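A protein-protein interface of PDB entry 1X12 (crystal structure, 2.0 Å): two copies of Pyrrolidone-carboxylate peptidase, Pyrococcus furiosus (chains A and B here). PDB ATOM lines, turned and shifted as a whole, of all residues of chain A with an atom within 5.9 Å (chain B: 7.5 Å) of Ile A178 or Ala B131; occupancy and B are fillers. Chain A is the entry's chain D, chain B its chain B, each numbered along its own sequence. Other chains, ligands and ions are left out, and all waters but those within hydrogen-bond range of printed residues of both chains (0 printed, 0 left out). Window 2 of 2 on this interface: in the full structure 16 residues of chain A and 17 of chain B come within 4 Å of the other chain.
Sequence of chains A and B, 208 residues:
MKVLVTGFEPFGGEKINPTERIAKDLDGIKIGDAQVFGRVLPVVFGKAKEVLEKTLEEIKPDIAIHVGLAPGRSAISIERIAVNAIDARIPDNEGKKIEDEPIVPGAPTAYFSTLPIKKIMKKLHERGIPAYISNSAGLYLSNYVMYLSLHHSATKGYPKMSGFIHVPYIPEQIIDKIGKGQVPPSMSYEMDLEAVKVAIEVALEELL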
ATOM      1  N   ILE A 174      19.138  26.768   2.173  1.00  0.00           N
ATOM      2  CA  ILE A 174      19.285  25.406   1.675  1.00  0.00           C
ATOM      3  C   ILE A 174      20.576  24.722   2.143  1.00  0.00           C
ATOM      4  O   ILE A 174      20.629  23.498   2.244  1.00  0.00           O
ATOM      5  CB  ILE A 174      19.257  25.386   0.123  1.00  0.00           C
ATOM      6  CG1 ILE A 174      17.984  26.066  -0.392  1.00  0.00           C
ATOM      7  CG2 ILE A 174      19.335  23.953  -0.386  1.00  0.00           C
ATOM      8  CD1 ILE A 174      16.696  25.401   0.058  1.00  0.00           C
ATOM      9  N   ILE A 175      21.603  25.509   2.444  1.00  0.00           N
ATOM     10  CA  ILE A 175      22.894  24.963   2.863  1.00  0.00           C
ATOM     11  C   ILE A 175      22.813  23.869   3.922  1.00  0.00           C
ATOM     12  O   ILE A 175      23.271  22.747   3.701  1.00  0.00           O
ATOM     13  CB  ILE A 175      23.834  26.078   3.374  1.00  0.00           C
ATOM     14  CG1 ILE A 175      23.968  27.173   2.307  1.00  0.00           C
ATOM     15  CG2 ILE A 175      25.198  25.495   3.713  1.00  0.00           C
ATOM     16  CD1 ILE A 175      24.339  26.654   0.927  1.00  0.00           C
ATOM     17  N   ASP A 176      22.230  24.184   5.073  1.00  0.00           N
ATOM     18  CA  ASP A 176      22.131  23.197   6.138  1.00  0.00           C
ATOM     19  C   ASP A 176      21.217  22.028   5.783  1.00  0.00           C
ATOM     20  O   ASP A 176      21.278  20.980   6.418  1.00  0.00           O
ATOM     21  CB  ASP A 176      21.665  23.861   7.436  1.00  0.00           C
ATOM     22  CG  ASP A 176      22.653  24.897   7.945  1.00  0.00           C
ATOM     23  OD1 ASP A 176      23.876  24.645   7.867  1.00  0.00           O
ATOM     24  OD2 ASP A 176      22.210  25.956   8.433  1.00  0.00           O
ATOM     25  N   LYS A 177      20.386  22.202   4.759  1.00  0.00           N
ATOM     26  CA  LYS A 177      19.470  21.148   4.323  1.00  0.00           C
ATOM     27  C   LYS A 177      20.245  20.056   3.594  1.00  0.00           C
ATOM     28  O   LYS A 177      19.856  18.886   3.609  1.00  0.00           O
ATOM     29  CB  LYS A 177      18.418  21.711   3.364  1.00  0.00           C
ATOM     30  CG  LYS A 177      17.696  22.954   3.855  1.00  0.00           C
ATOM     31  CD  LYS A 177      16.767  22.640   4.996  1.00  0.00           C
ATOM     32  CE  LYS A 177      16.029  23.888   5.437  1.00  0.00           C
ATOM     33  NZ  LYS A 177      15.019  23.552   6.464  1.00  0.00           N
ATOM     34  N   ILE A 178      21.332  20.458   2.941  1.00  0.00           N
ATOM     35  CA  ILE A 178      22.175  19.538   2.190  1.00  0.00           C
ATOM     36  C   ILE A 178      22.855  18.576   3.152  1.00  0.00           C
ATOM     37  O   ILE A 178      23.431  18.989   4.159  1.00  0.00           O
ATOM     38  CB  ILE A 178      23.247  20.302   1.382  1.00  0.00           C
ATOM     39  CG1 ILE A 178      22.564  21.291   0.432  1.00  0.00           C
ATOM     40  CG2 ILE A 178      24.105  19.319   0.591  1.00  0.00           C
ATOM     41  CD1 ILE A 178      23.519  22.185  -0.324  1.00  0.00           C
ATOM     42  N   GLY A 179      22.784  17.291   2.836  1.00  0.00           N
ATOM     43  CA  GLY A 179      23.387  16.299   3.703  1.00  0.00           C
ATOM     44  C   GLY A 179      22.283  15.722   4.564  1.00  0.00           C
ATOM     45  O   GLY A 179      22.275  14.525   4.864  1.00  0.00           O
ATOM     46  N   LYS A 180      21.344  16.580   4.959  1.00  0.00           N
ATOM     47  CA  LYS A 180      20.214  16.151   5.774  1.00  0.00           C
ATOM     48  C   LYS A 180      19.342  15.223   4.933  1.00  0.00           C
ATOM     49  O   LYS A 180      18.315  14.724   5.389  1.00  0.00           O
ATOM     50  CB  LYS A 180      19.396  17.359   6.259  1.00  0.00           C
ATOM     51  CG  LYS A 180      20.125  18.241   7.278  1.00  0.00           C
ATOM     52  CD  LYS A 180      19.277  19.434   7.716  1.00  0.00           C
ATOM     53  CE  LYS A 180      19.998  20.287   8.764  1.00  0.00           C
ATOM     54  NZ  LYS A 180      19.327  21.609   8.958  1.00  0.00           N
ATOM     55  N   GLY A 181      19.765  14.998   3.693  1.00  0.00           N
ATOM     56  CA  GLY A 181      19.035  14.104   2.817  1.00  0.00           C
ATOM     57  C   GLY A 181      18.040  14.745   1.876  1.00  0.00           C
ATOM     58  O   GLY A 181      17.047  14.112   1.526  1.00  0.00           O
ATOM     59  N   GLN A 182      18.285  15.985   1.459  1.00  0.00           N
ATOM     60  CA  GLN A 182      17.368  16.651   0.539  1.00  0.00           C
ATOM     61  C   GLN A 182      17.794  18.057   0.139  1.00  0.00           C
ATOM     62  O   GLN A 182      18.378  18.797   0.934  1.00  0.00           O
ATOM     63  CB  GLN A 182      15.961  16.722   1.134  1.00  0.00           C
ATOM     64  CG  GLN A 182      14.947  17.360   0.193  1.00  0.00           C
ATOM     65  CD  GLN A 182      14.709  16.529  -1.059  1.00  0.00           C
ATOM     66  OE1 GLN A 182      15.624  15.882  -1.577  1.00  0.00           O
ATOM     67  NE2 GLN A 182      13.477  16.555  -1.559  1.00  0.00           N
ATOM     68  N   VAL A 183      17.485  18.419  -1.103  1.00  0.00           N
ATOM     69  CA  VAL A 183      17.820  19.736  -1.616  1.00  0.00           C
ATOM     70  C   VAL A 183      16.558  20.414  -2.145  1.00  0.00           C
ATOM     71  O   VAL A 183      16.182  20.241  -3.308  1.00  0.00           O
ATOM     72  CB  VAL A 183      18.877  19.647  -2.738  1.00  0.00           C
ATOM     73  CG1 VAL A 183      19.388  21.036  -3.076  1.00  0.00           C
ATOM     74  CG2 VAL A 183      20.031  18.748  -2.299  1.00  0.00           C
ATOM     75  N   SER B  74      17.474  20.953  -8.313  1.00  0.00           N
ATOM     76  CA  SER B  74      17.256  22.159  -7.518  1.00  0.00           C
ATOM     77  C   SER B  74      18.484  22.921  -7.042  1.00  0.00           C
ATOM     78  O   SER B  74      18.356  24.008  -6.473  1.00  0.00           O
ATOM     79  CB  SER B  74      16.416  21.794  -6.299  1.00  0.00           C
ATOM     80  OG  SER B  74      17.105  20.825  -5.530  1.00  0.00           O
ATOM     81  N   ALA B  75      19.668  22.359  -7.246  1.00  0.00           N
ATOM     82  CA  ALA B  75      20.885  23.029  -6.812  1.00  0.00           C
ATOM     83  C   ALA B  75      22.053  22.603  -7.680  1.00  0.00           C
ATOM     84  O   ALA B  75      21.918  21.727  -8.535  1.00  0.00           O
ATOM     85  CB  ALA B  75      21.176  22.696  -5.350  1.00  0.00           C
ATOM     86  N   ILE B  76      23.200  23.236  -7.460  1.00  0.00           N
ATOM     87  CA  ILE B  76      24.405  22.900  -8.203  1.00  0.00           C
ATOM     88  C   ILE B  76      24.751  21.458  -7.847  1.00  0.00           C
ATOM     89  O   ILE B  76      24.692  21.076  -6.679  1.00  0.00           O
ATOM     90  CB  ILE B  76      25.595  23.805  -7.786  1.00  0.00           C
ATOM     91  CG1 ILE B  76      25.283  25.274  -8.096  1.00  0.00           C
ATOM     92  CG2 ILE B  76      26.868  23.363  -8.500  1.00  0.00           C
ATOM     93  CD1 ILE B  76      25.019  25.564  -9.569  1.00  0.00           C
ATOM     94  N   SER B  77      25.083  20.646  -8.845  1.00  0.00           N
ATOM     95  CA  SER B  77      25.460  19.265  -8.567  1.00  0.00           C
ATOM     96  C   SER B  77      26.798  18.958  -9.221  1.00  0.00           C
ATOM     97  O   SER B  77      27.033  19.297 -10.377  1.00  0.00           O
ATOM     98  CB  SER B  77      24.375  18.278  -9.038  1.00  0.00           C
ATOM     99  OG  SER B  77      24.023  18.463 -10.399  1.00  0.00           O
ATOM    100  N   ILE B  78      27.686  18.342  -8.445  1.00  0.00           N
ATOM    101  CA  ILE B  78      29.020  17.987  -8.908  1.00  0.00           C
ATOM    102  C   ILE B  78      29.041  16.481  -9.144  1.00  0.00           C
ATOM    103  O   ILE B  78      28.808  15.698  -8.223  1.00  0.00           O
ATOM    104  CB  ILE B  78      30.067  18.389  -7.844  1.00  0.00           C
ATOM    105  CG1 ILE B  78      29.865  19.864  -7.467  1.00  0.00           C
ATOM    106  CG2 ILE B  78      31.465  18.166  -8.382  1.00  0.00           C
ATOM    107  CD1 ILE B  78      30.491  20.259  -6.133  1.00  0.00           C
ATOM    108  N   ILE B 120      35.216  21.374  -3.344  1.00  0.00           N
ATOM    109  CA  ILE B 120      34.433  22.309  -4.139  1.00  0.00           C
ATOM    110  C   ILE B 120      33.058  22.504  -3.485  1.00  0.00           C
ATOM    111  O   ILE B 120      32.596  23.635  -3.310  1.00  0.00           O
ATOM    112  CB  ILE B 120      34.265  21.801  -5.589  1.00  0.00           C
ATOM    113  CG1 ILE B 120      35.619  21.843  -6.306  1.00  0.00           C
ATOM    114  CG2 ILE B 120      33.246  22.661  -6.337  1.00  0.00           C
ATOM    115  CD1 ILE B 120      35.606  21.259  -7.703  1.00  0.00           C
ATOM    116  N   MET B 121      32.416  21.398  -3.114  1.00  0.00           N
ATOM    117  CA  MET B 121      31.108  21.462  -2.476  1.00  0.00           C
ATOM    118  C   MET B 121      31.172  22.284  -1.190  1.00  0.00           C
ATOM    119  O   MET B 121      30.301  23.111  -0.927  1.00  0.00           O
ATOM    120  CB  MET B 121      30.590  20.051  -2.159  1.00  0.00           C
ATOM    121  CG  MET B 121      29.259  20.044  -1.408  1.00  0.00           C
ATOM    122  SD  MET B 121      28.519  18.401  -1.187  1.00  0.00           S
ATOM    123  CE  MET B 121      29.598  17.709   0.071  1.00  0.00           C
ATOM    124  N   LYS B 122      32.211  22.053  -0.397  1.00  0.00           N
ATOM    125  CA  LYS B 122      32.396  22.764   0.863  1.00  0.00           C
ATOM    126  C   LYS B 122      32.551  24.271   0.641  1.00  0.00           C
ATOM    127  O   LYS B 122      31.939  25.079   1.342  1.00  0.00           O
ATOM    128  CB  LYS B 122      33.627  22.204   1.591  1.00  0.00           C
ATOM    129  CG  LYS B 122      33.864  22.764   2.990  1.00  0.00           C
ATOM    130  CD  LYS B 122      34.449  24.164   2.953  1.00  0.00           C
ATOM    131  CE  LYS B 122      35.890  24.166   2.445  1.00  0.00           C
ATOM    132  NZ  LYS B 122      36.483  25.538   2.402  1.00  0.00           N
ATOM    133  N   LEU B 124      31.555  26.007  -1.941  1.00  0.00           N
ATOM    134  CA  LEU B 124      30.298  26.537  -2.446  1.00  0.00           C
ATOM    135  C   LEU B 124      29.356  26.807  -1.279  1.00  0.00           C
ATOM    136  O   LEU B 124      28.715  27.853  -1.225  1.00  0.00           O
ATOM    137  CB  LEU B 124      29.657  25.560  -3.435  1.00  0.00           C
ATOM    138  CG  LEU B 124      30.377  25.431  -4.781  1.00  0.00           C
ATOM    139  CD1 LEU B 124      29.738  24.324  -5.616  1.00  0.00           C
ATOM    140  CD2 LEU B 124      30.300  26.759  -5.523  1.00  0.00           C
ATOM    141  N   HIS B 125      29.286  25.865  -0.340  1.00  0.00           N
ATOM    142  CA  HIS B 125      28.429  26.024   0.831  1.00  0.00           C
ATOM    143  C   HIS B 125      28.829  27.255   1.640  1.00  0.00           C
ATOM    144  O   HIS B 125      27.972  27.997   2.123  1.00  0.00           O
ATOM    145  CB  HIS B 125      28.499  24.775   1.714  1.00  0.00           C
ATOM    146  CG  HIS B 125      27.842  23.573   1.111  1.00  0.00           C
ATOM    147  ND1 HIS B 125      27.814  22.346   1.737  1.00  0.00           N
ATOM    148  CD2 HIS B 125      27.173  23.415  -0.058  1.00  0.00           C
ATOM    149  CE1 HIS B 125      27.155  21.484   0.982  1.00  0.00           C
ATOM    150  NE2 HIS B 125      26.756  22.108  -0.112  1.00  0.00           N
ATOM    151  N   GLY B 128      27.365  30.233   0.411  1.00  0.00           N
ATOM    152  CA  GLY B 128      25.914  30.276   0.426  1.00  0.00           C
ATOM    153  C   GLY B 128      25.300  29.723  -0.848  1.00  0.00           C
ATOM    154  O   GLY B 128      24.166  30.052  -1.204  1.00  0.00           O
ATOM    155  N   ILE B 129      26.055  28.876  -1.539  1.00  0.00           N
ATOM    156  CA  ILE B 129      25.579  28.270  -2.771  1.00  0.00           C
ATOM    157  C   ILE B 129      25.224  26.807  -2.527  1.00  0.00           C
ATOM    158  O   ILE B 129      26.100  25.984  -2.265  1.00  0.00           O
ATOM    159  CB  ILE B 129      26.658  28.353  -3.871  1.00  0.00           C
ATOM    160  CG1 ILE B 129      26.956  29.825  -4.179  1.00  0.00           C
ATOM    161  CG2 ILE B 129      26.190  27.608  -5.128  1.00  0.00           C
ATOM    162  CD1 ILE B 129      28.098  30.044  -5.156  1.00  0.00           C
ATOM    163  N   PRO B 130      23.927  26.466  -2.593  1.00  0.00           N
ATOM    164  CA  PRO B 130      23.549  25.068  -2.368  1.00  0.00           C
ATOM    165  C   PRO B 130      24.139  24.184  -3.462  1.00  0.00           C
ATOM    166  O   PRO B 130      24.017  24.478  -4.652  1.00  0.00           O
ATOM    167  CB  PRO B 130      22.021  25.109  -2.387  1.00  0.00           C
ATOM    168  CG  PRO B 130      21.712  26.297  -3.234  1.00  0.00           C
ATOM    169  CD  PRO B 130      22.741  27.308  -2.814  1.00  0.00           C
ATOM    170  N   ALA B 131      24.791  23.109  -3.046  1.00  0.00           N
ATOM    171  CA  ALA B 131      25.424  22.198  -3.984  1.00  0.00           C
ATOM    172  C   ALA B 131      25.556  20.834  -3.335  1.00  0.00           C
ATOM    173  O   ALA B 131      25.681  20.730  -2.113  1.00  0.00           O
ATOM    174  CB  ALA B 131      26.800  22.730  -4.366  1.00  0.00           C
ATOM    175  N   TYR B 132      25.530  19.789  -4.151  1.00  0.00           N
ATOM    176  CA  TYR B 132      25.657  18.439  -3.634  1.00  0.00           C
ATOM    177  C   TYR B 132      26.360  17.558  -4.656  1.00  0.00           C
ATOM    178  O   TYR B 132      26.550  17.955  -5.806  1.00  0.00           O
ATOM    179  CB  TYR B 132      24.274  17.871  -3.296  1.00  0.00           C
ATOM    180  CG  TYR B 132      23.377  17.661  -4.496  1.00  0.00           C
ATOM    181  CD1 TYR B 132      23.290  16.417  -5.115  1.00  0.00           C
ATOM    182  CD2 TYR B 132      22.616  18.710  -5.013  1.00  0.00           C
ATOM    183  CE1 TYR B 132      22.460  16.217  -6.221  1.00  0.00           C
ATOM    184  CE2 TYR B 132      21.785  18.523  -6.117  1.00  0.00           C
ATOM    185  CZ  TYR B 132      21.713  17.274  -6.713  1.00  0.00           C
ATOM    186  OH  TYR B 132      20.879  17.077  -7.788  1.00  0.00           O
ATOM    187  N   ILE B 133      26.756  16.368  -4.222  1.00  0.00           N
ATOM    188  CA  ILE B 133      27.447  15.436  -5.099  1.00  0.00           C
ATOM    189  C   ILE B 133      26.435  14.530  -5.793  1.00  0.00           C
ATOM    190  O   ILE B 133      25.627  13.878  -5.132  1.00  0.00           O
ATOM    191  CB  ILE B 133      28.425  14.537  -4.307  1.00  0.00           C
ATOM    192  CG1 ILE B 133      29.419  15.395  -3.518  1.00  0.00           C
ATOM    193  CG2 ILE B 133      29.151  13.591  -5.258  1.00  0.00           C
ATOM    194  CD1 ILE B 133      30.226  16.362  -4.358  1.00  0.00           C
ATOM    195  N   SER B 134      26.476  14.502  -7.120  1.00  0.00           N
ATOM    196  CA  SER B 134      25.591  13.644  -7.901  1.00  0.00           C
ATOM    197  C   SER B 134      26.345  12.364  -8.246  1.00  0.00           C
ATOM    198  O   SER B 134      27.531  12.407  -8.587  1.00  0.00           O
ATOM    199  CB  SER B 134      25.157  14.339  -9.192  1.00  0.00           C
ATOM    200  OG  SER B 134      24.531  13.419 -10.073  1.00  0.00           O
ATOM    201  N   MET B 187      17.616  28.215 -10.504  1.00  0.00           N
ATOM    202  CA  MET B 187      18.696  28.884  -9.785  1.00  0.00           C
ATOM    203  C   MET B 187      19.217  29.999 -10.689  1.00  0.00           C
ATOM    204  O   MET B 187      19.331  29.820 -11.899  1.00  0.00           O
ATOM    205  CB  MET B 187      19.811  27.885  -9.452  1.00  0.00           C
ATOM    206  CG  MET B 187      20.969  28.488  -8.665  1.00  0.00           C
ATOM    207  SD  MET B 187      22.075  27.223  -8.022  1.00  0.00           S
ATOM    208  CE  MET B 187      21.228  26.773  -6.501  1.00  0.00           C
ATOM    209  N   ALA B 195      29.494  29.814  -9.031  1.00  0.00           N
ATOM    210  CA  ALA B 195      29.761  28.433  -8.639  1.00  0.00           C
ATOM    211  C   ALA B 195      30.873  27.836  -9.495  1.00  0.00           C
ATOM    212  O   ALA B 195      31.775  27.174  -8.979  1.00  0.00           O
ATOM    213  CB  ALA B 195      28.493  27.588  -8.771  1.00  0.00           C
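No position is printed for both chains.
Of the 19 printed residues of chain B, 8 touch a printed residue of chain A. Hydrophobic or aromatic side chains of chain B that line the printed part of chain A: Ala B75, His B125, Pro B130 and Tyr B132. Along chain A the printed residues that touch a printed residue of chain B span positions 174 to 183. Among the printed residues, 11 pairs touch across the chains.
Of the printed residues of chain B, Val A183 touches Ser B74 (2.5 Å), Ala B75 (3.3 Å) and Tyr B132 (3.7 Å). Printed residues of chain A within 4 Å of Gly B128: Ile A175. Of the printed residues of chain A, Ile B129 touches Ile A175. Of chain A, only Ile A178 comes within 4 Å of Ala B131. Printed residues of chain A within 4 Å of Tyr B132: Val A183. The nearest residue of chain A that does not touch Ala B131 is Ile A175 (5.3 Å). The nearest printed residue of chain B that does not touch Ile A175 is Leu B124 (5.0 Å).
Among the printed residues, pairs that only touch across the chains: Ile A178 with Ala B131, Ile A178 with His B125, Val A183 with Ala B75, Ile A178 with Pro B130, Ile A174 with Pro B130, Ile A175 with Pro B130, Ile A175 with Ile B129, Ile A175 with Gly B128, Val A183 with Tyr B132 and Ile A175 with His B125.
The backbone carbonyl oxygen of Val A183 sits at hydrogen-bond distance from the side-chain hydroxyl of Ser B74 (2.5 Å).
The backbone NH (N) of Ile B76 lies within hydrogen-bond range of the backbone carbonyl oxygen (O) of Pro B130, 3.2 Å away. N of Tyr B132 sits at hydrogen-bond distance from O of Ile B76 (3.0 Å). The backbone NH (N) of Ile B78 is in hydrogen-bond range of the backbone carbonyl oxygen (O) of Tyr B132 (2.9 Å). The backbone NH (N) of Ile B129 lies within hydrogen-bond range of the backbone carbonyl oxygen (O) of Leu B124 (2.9 Å). A ring nitrogen (NE2) of His B125 sits at hydrogen-bond distance from the backbone carbonyl oxygen (O) of Ala B131 (2.7 Å).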
